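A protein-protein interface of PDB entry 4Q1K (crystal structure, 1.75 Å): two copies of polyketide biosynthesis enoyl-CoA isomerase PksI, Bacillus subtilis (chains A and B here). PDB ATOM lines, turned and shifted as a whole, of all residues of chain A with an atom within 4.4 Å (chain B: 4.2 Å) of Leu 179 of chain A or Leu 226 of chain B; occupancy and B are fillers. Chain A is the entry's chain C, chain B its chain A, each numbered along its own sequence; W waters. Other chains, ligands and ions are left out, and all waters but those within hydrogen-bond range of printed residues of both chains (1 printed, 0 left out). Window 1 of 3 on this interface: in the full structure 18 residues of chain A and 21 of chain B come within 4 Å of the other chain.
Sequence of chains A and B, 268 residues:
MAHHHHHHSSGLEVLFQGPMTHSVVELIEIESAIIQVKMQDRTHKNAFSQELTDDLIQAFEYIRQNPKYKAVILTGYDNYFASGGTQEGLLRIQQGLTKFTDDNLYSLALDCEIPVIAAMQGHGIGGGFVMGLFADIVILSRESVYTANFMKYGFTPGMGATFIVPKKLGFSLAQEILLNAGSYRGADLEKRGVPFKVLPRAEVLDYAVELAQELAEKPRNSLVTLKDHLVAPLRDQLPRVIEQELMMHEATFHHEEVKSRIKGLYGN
Of the 12 printed residues of chain A, 9 touch a printed residue of chain B.
Among the printed residues, no Asp or Glu carboxylate lies within 4 Å of a Lys or Arg side-chain nitrogen of the other chain.
Water W1 bridges the side-chain amide oxygen (OE1) of Gln 175 of chain A (3.1 Å) and the backbone carbonyl oxygen (O) of Leu 230 of chain B (3.2 Å).
No position is printed for both chains.
Printed residues of chain B within 4 Å of Thr 162 of chain A: Leu 226 (3.99 Å) and His 229 (2.8 Å).
Of chain B, only Leu 215, Lys 218 and Leu 226 come within 4 Å of Leu 179 of chain A.
Of the printed residues of chain A, Leu 215 of chain B touches Leu 179 and Asn 180.
Of the printed residues of chain A, Lys 218 of chain B touches Met 151, Leu 179 and Asn 180.
The nearest residue of chain B that does not touch Leu 179 of chain A is Leu 230 of chain B (4.04 Å).
The nearest printed residue of chain B that does not touch Pro 157 of chain A is His 229 of chain B (6.5 Å).
Among the printed residues, pairs that only touch across the chains: Met 151 of chain A with Lys 218 of chain B, Met 151 of chain A with Ser 222 of chain B, Met 151 of chain A with Leu 223 of chain B, Met 151 of chain A with Leu 226 of chain B, Thr 156 of chain A with Ser 222 of chain B, Pro 157 of chain A with Leu 226 of chain B, Thr 162 of chain A with Leu 226 of chain B, Gln 175 of chain A with Leu 230 of chain B, Leu 178 of chain A with Leu 226 of chain B, Leu 178 of chain A with Leu 230 of chain B, Leu 179 of chain A with Leu 215 of chain B, Leu 179 of chain A with Lys 218 of chain B, Leu 179 of chain A with Leu 226 of chain B and Met 248 of chain A with His 229 of chain B.
The side-chain amino group (NZ) of Lys 218 of chain B is in hydrogen-bond range of the backbone carbonyl oxygen (O) of Asn 180 of chain A (2.9 Å).
NE2 of His 229 of chain B is in hydrogen-bond range of OG1 of Thr 162 of chain A (2.8 Å).
The backbone NH of Leu 215 of chain B lies within hydrogen-bond range of the side-chain amide oxygen of Asn 180 of chain A (3.4 Å).
SD of Met 248 of chain A lies close to O of Thr 225 of chain B (3.7 Å).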
ATOM      1  N   MET A 151     -16.018  25.524 -24.498  1.00  0.00           N
ATOM      2  CA  MET A 151     -16.591  26.740 -25.040  1.00  0.00           C
ATOM      3  C   MET A 151     -18.120  26.683 -24.965  1.00  0.00           C
ATOM      4  O   MET A 151     -18.771  27.727 -25.006  1.00  0.00           O
ATOM      5  CB  MET A 151     -16.134  27.029 -26.463  1.00  0.00           C
ATOM      6  CG  MET A 151     -14.627  27.437 -26.487  1.00  0.00           C
ATOM      7  SD  MET A 151     -14.468  29.254 -26.188  1.00  0.00           S
ATOM      8  CE  MET A 151     -14.953  29.943 -27.797  1.00  0.00           C
ATOM      9  N   THR A 156     -12.828  29.654 -22.371  1.00  0.00           N
ATOM     10  CA  THR A 156     -11.880  29.103 -23.349  1.00  0.00           C
ATOM     11  C   THR A 156     -11.330  27.773 -22.844  1.00  0.00           C
ATOM     12  O   THR A 156     -11.286  27.480 -21.656  1.00  0.00           O
ATOM     13  CB  THR A 156     -10.736  30.146 -23.543  1.00  0.00           C
ATOM     14  OG1 THR A 156     -10.256  30.577 -22.254  1.00  0.00           O
ATOM     15  CG2 THR A 156     -11.307  31.356 -24.328  1.00  0.00           C
ATOM     16  N   PRO A 157     -10.848  26.925 -23.733  1.00  0.00           N
ATOM     17  CA  PRO A 157     -10.381  25.616 -23.300  1.00  0.00           C
ATOM     18  C   PRO A 157      -9.092  25.673 -22.440  1.00  0.00           C
ATOM     19  O   PRO A 157      -8.171  26.446 -22.747  1.00  0.00           O
ATOM     20  CB  PRO A 157     -10.056  24.929 -24.627  1.00  0.00           C
ATOM     21  CG  PRO A 157     -10.823  25.649 -25.682  1.00  0.00           C
ATOM     22  CD  PRO A 157     -10.894  27.098 -25.200  1.00  0.00           C
ATOM     23  N   THR A 162      -5.483  23.428 -25.910  1.00  0.00           N
ATOM     24  CA  THR A 162      -5.167  24.167 -27.121  1.00  0.00           C
ATOM     25  C   THR A 162      -3.824  23.715 -27.648  1.00  0.00           C
ATOM     26  O   THR A 162      -3.387  24.075 -28.736  1.00  0.00           O
ATOM     27  CB  THR A 162      -5.224  25.715 -26.873  1.00  0.00           C
ATOM     28  OG1 THR A 162      -4.212  26.102 -25.959  1.00  0.00           O
ATOM     29  CG2 THR A 162      -6.586  26.126 -26.314  1.00  0.00           C
ATOM     30  N   GLN A 175      -9.149  23.418 -34.747  1.00  0.00           N
ATOM     31  CA  GLN A 175      -9.886  24.678 -34.776  1.00  0.00           C
ATOM     32  C   GLN A 175     -11.415  24.454 -34.552  1.00  0.00           C
ATOM     33  O   GLN A 175     -12.041  25.136 -33.730  1.00  0.00           O
ATOM     34  CB  GLN A 175      -9.670  25.539 -36.063  1.00  0.00           C
ATOM     35  CG  GLN A 175      -8.243  25.693 -36.490  1.00  0.00           C
ATOM     36  CD  GLN A 175      -7.405  26.223 -35.362  1.00  0.00           C
ATOM     37  OE1 GLN A 175      -6.618  25.474 -34.716  1.00  0.00           O
ATOM     38  NE2 GLN A 175      -7.574  27.523 -35.076  1.00  0.00           N
ATOM     39  N   GLU A 176     -12.017  23.541 -35.313  1.00  0.00           N
ATOM     40  CA  GLU A 176     -13.437  23.242 -35.220  1.00  0.00           C
ATOM     41  C   GLU A 176     -13.793  22.634 -33.873  1.00  0.00           C
ATOM     42  O   GLU A 176     -14.724  23.072 -33.199  1.00  0.00           O
ATOM     43  CB  GLU A 176     -13.754  22.232 -36.369  1.00  0.00           C
ATOM     44  CG  GLU A 176     -15.204  21.852 -36.403  1.00  0.00           C
ATOM     45  CD  GLU A 176     -15.396  20.730 -37.432  1.00  0.00           C
ATOM     46  OE1 GLU A 176     -14.793  20.855 -38.531  1.00  0.00           O
ATOM     47  OE2 GLU A 176     -16.040  19.714 -37.048  1.00  0.00           O
ATOM     48  N   ILE A 177     -12.978  21.679 -33.414  1.00  0.00           N
ATOM     49  CA  ILE A 177     -13.239  21.072 -32.077  1.00  0.00           C
ATOM     50  C   ILE A 177     -13.218  22.094 -30.938  1.00  0.00           C
ATOM     51  O   ILE A 177     -14.131  22.084 -30.102  1.00  0.00           O
ATOM     52  CB  ILE A 177     -12.198  19.955 -31.820  1.00  0.00           C
ATOM     53  CG1 ILE A 177     -12.557  18.782 -32.775  1.00  0.00           C
ATOM     54  CG2 ILE A 177     -12.177  19.470 -30.334  1.00  0.00           C
ATOM     55  CD1 ILE A 177     -11.487  17.704 -32.772  1.00  0.00           C
ATOM     56  N   LEU A 178     -12.199  22.959 -30.943  1.00  0.00           N
ATOM     57  CA  LEU A 178     -12.040  23.885 -29.812  1.00  0.00           C
ATOM     58  C   LEU A 178     -12.996  25.074 -29.901  1.00  0.00           C
ATOM     59  O   LEU A 178     -13.563  25.446 -28.874  1.00  0.00           O
ATOM     60  CB  LEU A 178     -10.581  24.353 -29.819  1.00  0.00           C
ATOM     61  CG  LEU A 178      -9.643  23.190 -29.464  1.00  0.00           C
ATOM     62  CD1 LEU A 178      -8.256  23.712 -29.725  1.00  0.00           C
ATOM     63  CD2 LEU A 178      -9.612  22.673 -27.991  1.00  0.00           C
ATOM     64  N   LEU A 179     -13.153  25.692 -31.082  1.00  0.00           N
ATOM     65  CA  LEU A 179     -13.999  26.912 -31.164  1.00  0.00           C
ATOM     66  C   LEU A 179     -15.447  26.525 -30.930  1.00  0.00           C
ATOM     67  O   LEU A 179     -16.256  27.292 -30.306  1.00  0.00           O
ATOM     68  CB  LEU A 179     -13.882  27.629 -32.570  1.00  0.00           C
ATOM     69  CG  LEU A 179     -12.496  28.282 -32.823  1.00  0.00           C
ATOM     70  CD1 LEU A 179     -12.453  28.535 -34.326  1.00  0.00           C
ATOM     71  CD2 LEU A 179     -12.652  29.601 -32.078  1.00  0.00           C
ATOM     72  N   ASN A 180     -15.827  25.371 -31.487  1.00  0.00           N
ATOM     73  CA  ASN A 180     -17.250  25.083 -31.561  1.00  0.00           C
ATOM     74  C   ASN A 180     -17.768  24.151 -30.454  1.00  0.00           C
ATOM     75  O   ASN A 180     -18.995  24.095 -30.182  1.00  0.00           O
ATOM     76  CB  ASN A 180     -17.687  24.593 -32.952  1.00  0.00           C
ATOM     77  CG  ASN A 180     -19.155  24.671 -33.113  1.00  0.00           C
ATOM     78  OD1 ASN A 180     -19.757  25.666 -32.713  1.00  0.00           O
ATOM     79  ND2 ASN A 180     -19.763  23.592 -33.612  1.00  0.00           N
ATOM     80  N   ALA A 181     -16.858  23.479 -29.780  1.00  0.00           N
ATOM     81  CA  ALA A 181     -17.211  22.654 -28.590  1.00  0.00           C
ATOM     82  C   ALA A 181     -18.278  21.590 -28.987  1.00  0.00           C
ATOM     83  O   ALA A 181     -19.008  21.113 -28.131  1.00  0.00           O
ATOM     84  CB  ALA A 181     -17.724  23.558 -27.427  1.00  0.00           C
ATOM     85  N   MET A 248      -6.057  33.282 -20.896  1.00  0.00           N
ATOM     86  CA  MET A 248      -7.388  33.298 -21.506  1.00  0.00           C
ATOM     87  C   MET A 248      -8.460  33.066 -20.500  1.00  0.00           C
ATOM     88  O   MET A 248      -9.538  33.642 -20.665  1.00  0.00           O
ATOM     89  CB  MET A 248      -7.530  32.248 -22.680  1.00  0.00           C
ATOM     90  CG  MET A 248      -6.643  32.601 -23.854  1.00  0.00           C
ATOM     91  SD  MET A 248      -7.135  31.587 -25.272  1.00  0.00           S
ATOM     92  CE  MET A 248      -6.584  29.946 -24.708  1.00  0.00           C
ATOM     93  N   LEU B 215     -21.586  28.356 -33.629  1.00  0.00           N
ATOM     94  CA  LEU B 215     -20.526  29.239 -33.151  1.00  0.00           C
ATOM     95  C   LEU B 215     -21.193  30.430 -32.465  1.00  0.00           C
ATOM     96  O   LEU B 215     -20.676  30.897 -31.404  1.00  0.00           O
ATOM     97  CB  LEU B 215     -19.634  29.767 -34.255  1.00  0.00           C
ATOM     98  CG  LEU B 215     -18.683  28.662 -34.808  1.00  0.00           C
ATOM     99  CD1 LEU B 215     -18.060  29.026 -36.164  1.00  0.00           C
ATOM    100  CD2 LEU B 215     -17.569  28.361 -33.787  1.00  0.00           C
ATOM    101  N   LYS B 218     -21.831  31.122 -28.650  1.00  0.00           N
ATOM    102  CA  LYS B 218     -20.718  31.386 -27.726  1.00  0.00           C
ATOM    103  C   LYS B 218     -20.637  32.911 -27.488  1.00  0.00           C
ATOM    104  O   LYS B 218     -21.013  33.707 -28.416  1.00  0.00           O
ATOM    105  CB  LYS B 218     -19.381  30.946 -28.332  1.00  0.00           C
ATOM    106  CG  LYS B 218     -19.062  29.447 -28.145  1.00  0.00           C
ATOM    107  CD  LYS B 218     -20.107  28.514 -28.779  1.00  0.00           C
ATOM    108  CE  LYS B 218     -19.504  27.136 -29.177  1.00  0.00           C
ATOM    109  NZ  LYS B 218     -20.647  26.385 -29.788  1.00  0.00           N
ATOM    110  N   SER B 222     -15.296  35.353 -26.061  1.00  0.00           N
ATOM    111  CA  SER B 222     -14.555  34.038 -25.902  1.00  0.00           C
ATOM    112  C   SER B 222     -14.123  33.550 -27.308  1.00  0.00           C
ATOM    113  O   SER B 222     -13.011  33.005 -27.454  1.00  0.00           O
ATOM    114  CB  SER B 222     -15.495  32.978 -25.304  1.00  0.00           C
ATOM    115  OG  SER B 222     -15.717  33.344 -23.976  1.00  0.00           O
ATOM    116  N   LEU B 223     -15.004  33.731 -28.311  1.00  0.00           N
ATOM    117  CA  LEU B 223     -14.619  33.378 -29.739  1.00  0.00           C
ATOM    118  C   LEU B 223     -13.328  34.138 -30.154  1.00  0.00           C
ATOM    119  O   LEU B 223     -12.392  33.574 -30.726  1.00  0.00           O
ATOM    120  CB  LEU B 223     -15.724  33.679 -30.775  1.00  0.00           C
ATOM    121  CG  LEU B 223     -16.989  32.842 -30.533  1.00  0.00           C
ATOM    122  CD1 LEU B 223     -18.123  33.376 -31.369  1.00  0.00           C
ATOM    123  CD2 LEU B 223     -16.715  31.363 -31.041  1.00  0.00           C
ATOM    124  N   VAL B 224     -13.336  35.480 -29.934  1.00  0.00           N
ATOM    125  CA  VAL B 224     -12.207  36.270 -30.329  1.00  0.00           C
ATOM    126  C   VAL B 224     -10.926  35.923 -29.552  1.00  0.00           C
ATOM    127  O   VAL B 224      -9.852  35.816 -30.135  1.00  0.00           O
ATOM    128  CB  VAL B 224     -12.548  37.797 -30.205  1.00  0.00           C
ATOM    129  CG1 VAL B 224     -11.327  38.577 -30.593  1.00  0.00           C
ATOM    130  CG2 VAL B 224     -13.732  38.090 -31.157  1.00  0.00           C
ATOM    131  N   THR B 225     -11.062  35.780 -28.228  1.00  0.00           N
ATOM    132  CA  THR B 225      -9.908  35.438 -27.325  1.00  0.00           C
ATOM    133  C   THR B 225      -9.301  34.118 -27.797  1.00  0.00           C
ATOM    134  O   THR B 225      -8.069  33.989 -27.971  1.00  0.00           O
ATOM    135  CB  THR B 225     -10.438  35.336 -25.903  1.00  0.00           C
ATOM    136  OG1 THR B 225     -10.779  36.687 -25.464  1.00  0.00           O
ATOM    137  CG2 THR B 225      -9.356  34.881 -24.999  1.00  0.00           C
ATOM    138  N   LEU B 226     -10.182  33.139 -28.028  1.00  0.00           N
ATOM    139  CA  LEU B 226      -9.660  31.823 -28.494  1.00  0.00           C
ATOM    140  C   LEU B 226      -9.045  31.881 -29.886  1.00  0.00           C
ATOM    141  O   LEU B 226      -7.939  31.326 -30.130  1.00  0.00           O
ATOM    142  CB  LEU B 226     -10.812  30.732 -28.363  1.00  0.00           C
ATOM    143  CG  LEU B 226     -10.277  29.311 -28.740  1.00  0.00           C
ATOM    144  CD1 LEU B 226      -9.031  28.875 -27.864  1.00  0.00           C
ATOM    145  CD2 LEU B 226     -11.499  28.301 -28.644  1.00  0.00           C
ATOM    146  N   LYS B 227      -9.727  32.507 -30.841  1.00  0.00           N
ATOM    147  CA  LYS B 227      -9.183  32.583 -32.178  1.00  0.00           C
ATOM    148  C   LYS B 227      -7.848  33.306 -32.119  1.00  0.00           C
ATOM    149  O   LYS B 227      -6.870  32.852 -32.757  1.00  0.00           O
ATOM    150  CB  LYS B 227     -10.153  33.298 -33.170  1.00  0.00           C
ATOM    151  CG  LYS B 227      -9.410  33.440 -34.537  1.00  0.00           C
ATOM    152  CD  LYS B 227     -10.364  34.050 -35.606  1.00  0.00           C
ATOM    153  CE  LYS B 227      -9.497  34.232 -36.887  1.00  0.00           C
ATOM    154  NZ  LYS B 227     -10.401  34.469 -38.097  1.00  0.00           N
ATOM    155  N   ASP B 228      -7.762  34.448 -31.417  1.00  0.00           N
ATOM    156  CA  ASP B 228      -6.430  35.144 -31.320  1.00  0.00           C
ATOM    157  C   ASP B 228      -5.326  34.176 -30.874  1.00  0.00           C
ATOM    158  O   ASP B 228      -4.189  34.201 -31.395  1.00  0.00           O
ATOM    159  CB  ASP B 228      -6.434  36.320 -30.291  1.00  0.00           C
ATOM    160  CG  ASP B 228      -7.128  37.569 -30.810  1.00  0.00           C
ATOM    161  OD1 ASP B 228      -7.378  37.727 -32.032  1.00  0.00           O
ATOM    162  OD2 ASP B 228      -7.458  38.434 -29.938  1.00  0.00           O
ATOM    163  N   HIS B 229      -5.624  33.348 -29.892  1.00  0.00           N
ATOM    164  CA  HIS B 229      -4.618  32.439 -29.363  1.00  0.00           C
ATOM    165  C   HIS B 229      -4.325  31.329 -30.398  1.00  0.00           C
ATOM    166  O   HIS B 229      -3.154  30.952 -30.660  1.00  0.00           O
ATOM    167  CB  HIS B 229      -5.169  31.796 -28.069  1.00  0.00           C
ATOM    168  CG  HIS B 229      -4.366  30.620 -27.526  1.00  0.00           C
ATOM    169  ND1 HIS B 229      -3.131  30.770 -26.911  1.00  0.00           N
ATOM    170  CD2 HIS B 229      -4.641  29.286 -27.475  1.00  0.00           C
ATOM    171  CE1 HIS B 229      -2.714  29.610 -26.464  1.00  0.00           C
ATOM    172  NE2 HIS B 229      -3.601  28.686 -26.793  1.00  0.00           N
ATOM    173  N   LEU B 230      -5.369  30.784 -30.990  1.00  0.00           N
ATOM    174  CA  LEU B 230      -5.098  29.614 -31.903  1.00  0.00           C
ATOM    175  C   LEU B 230      -4.324  30.008 -33.194  1.00  0.00           C
ATOM    176  O   LEU B 230      -3.559  29.225 -33.723  1.00  0.00           O
ATOM    177  CB  LEU B 230      -6.442  29.011 -32.368  1.00  0.00           C
ATOM    178  CG  LEU B 230      -7.230  28.334 -31.252  1.00  0.00           C
ATOM    179  CD1 LEU B 230      -8.623  27.872 -31.759  1.00  0.00           C
ATOM    180  CD2 LEU B 230      -6.497  27.199 -30.543  1.00  0.00           C
HETATM  181  O   HOH W   1      -4.061  26.172 -33.043  1.00  0.00           O
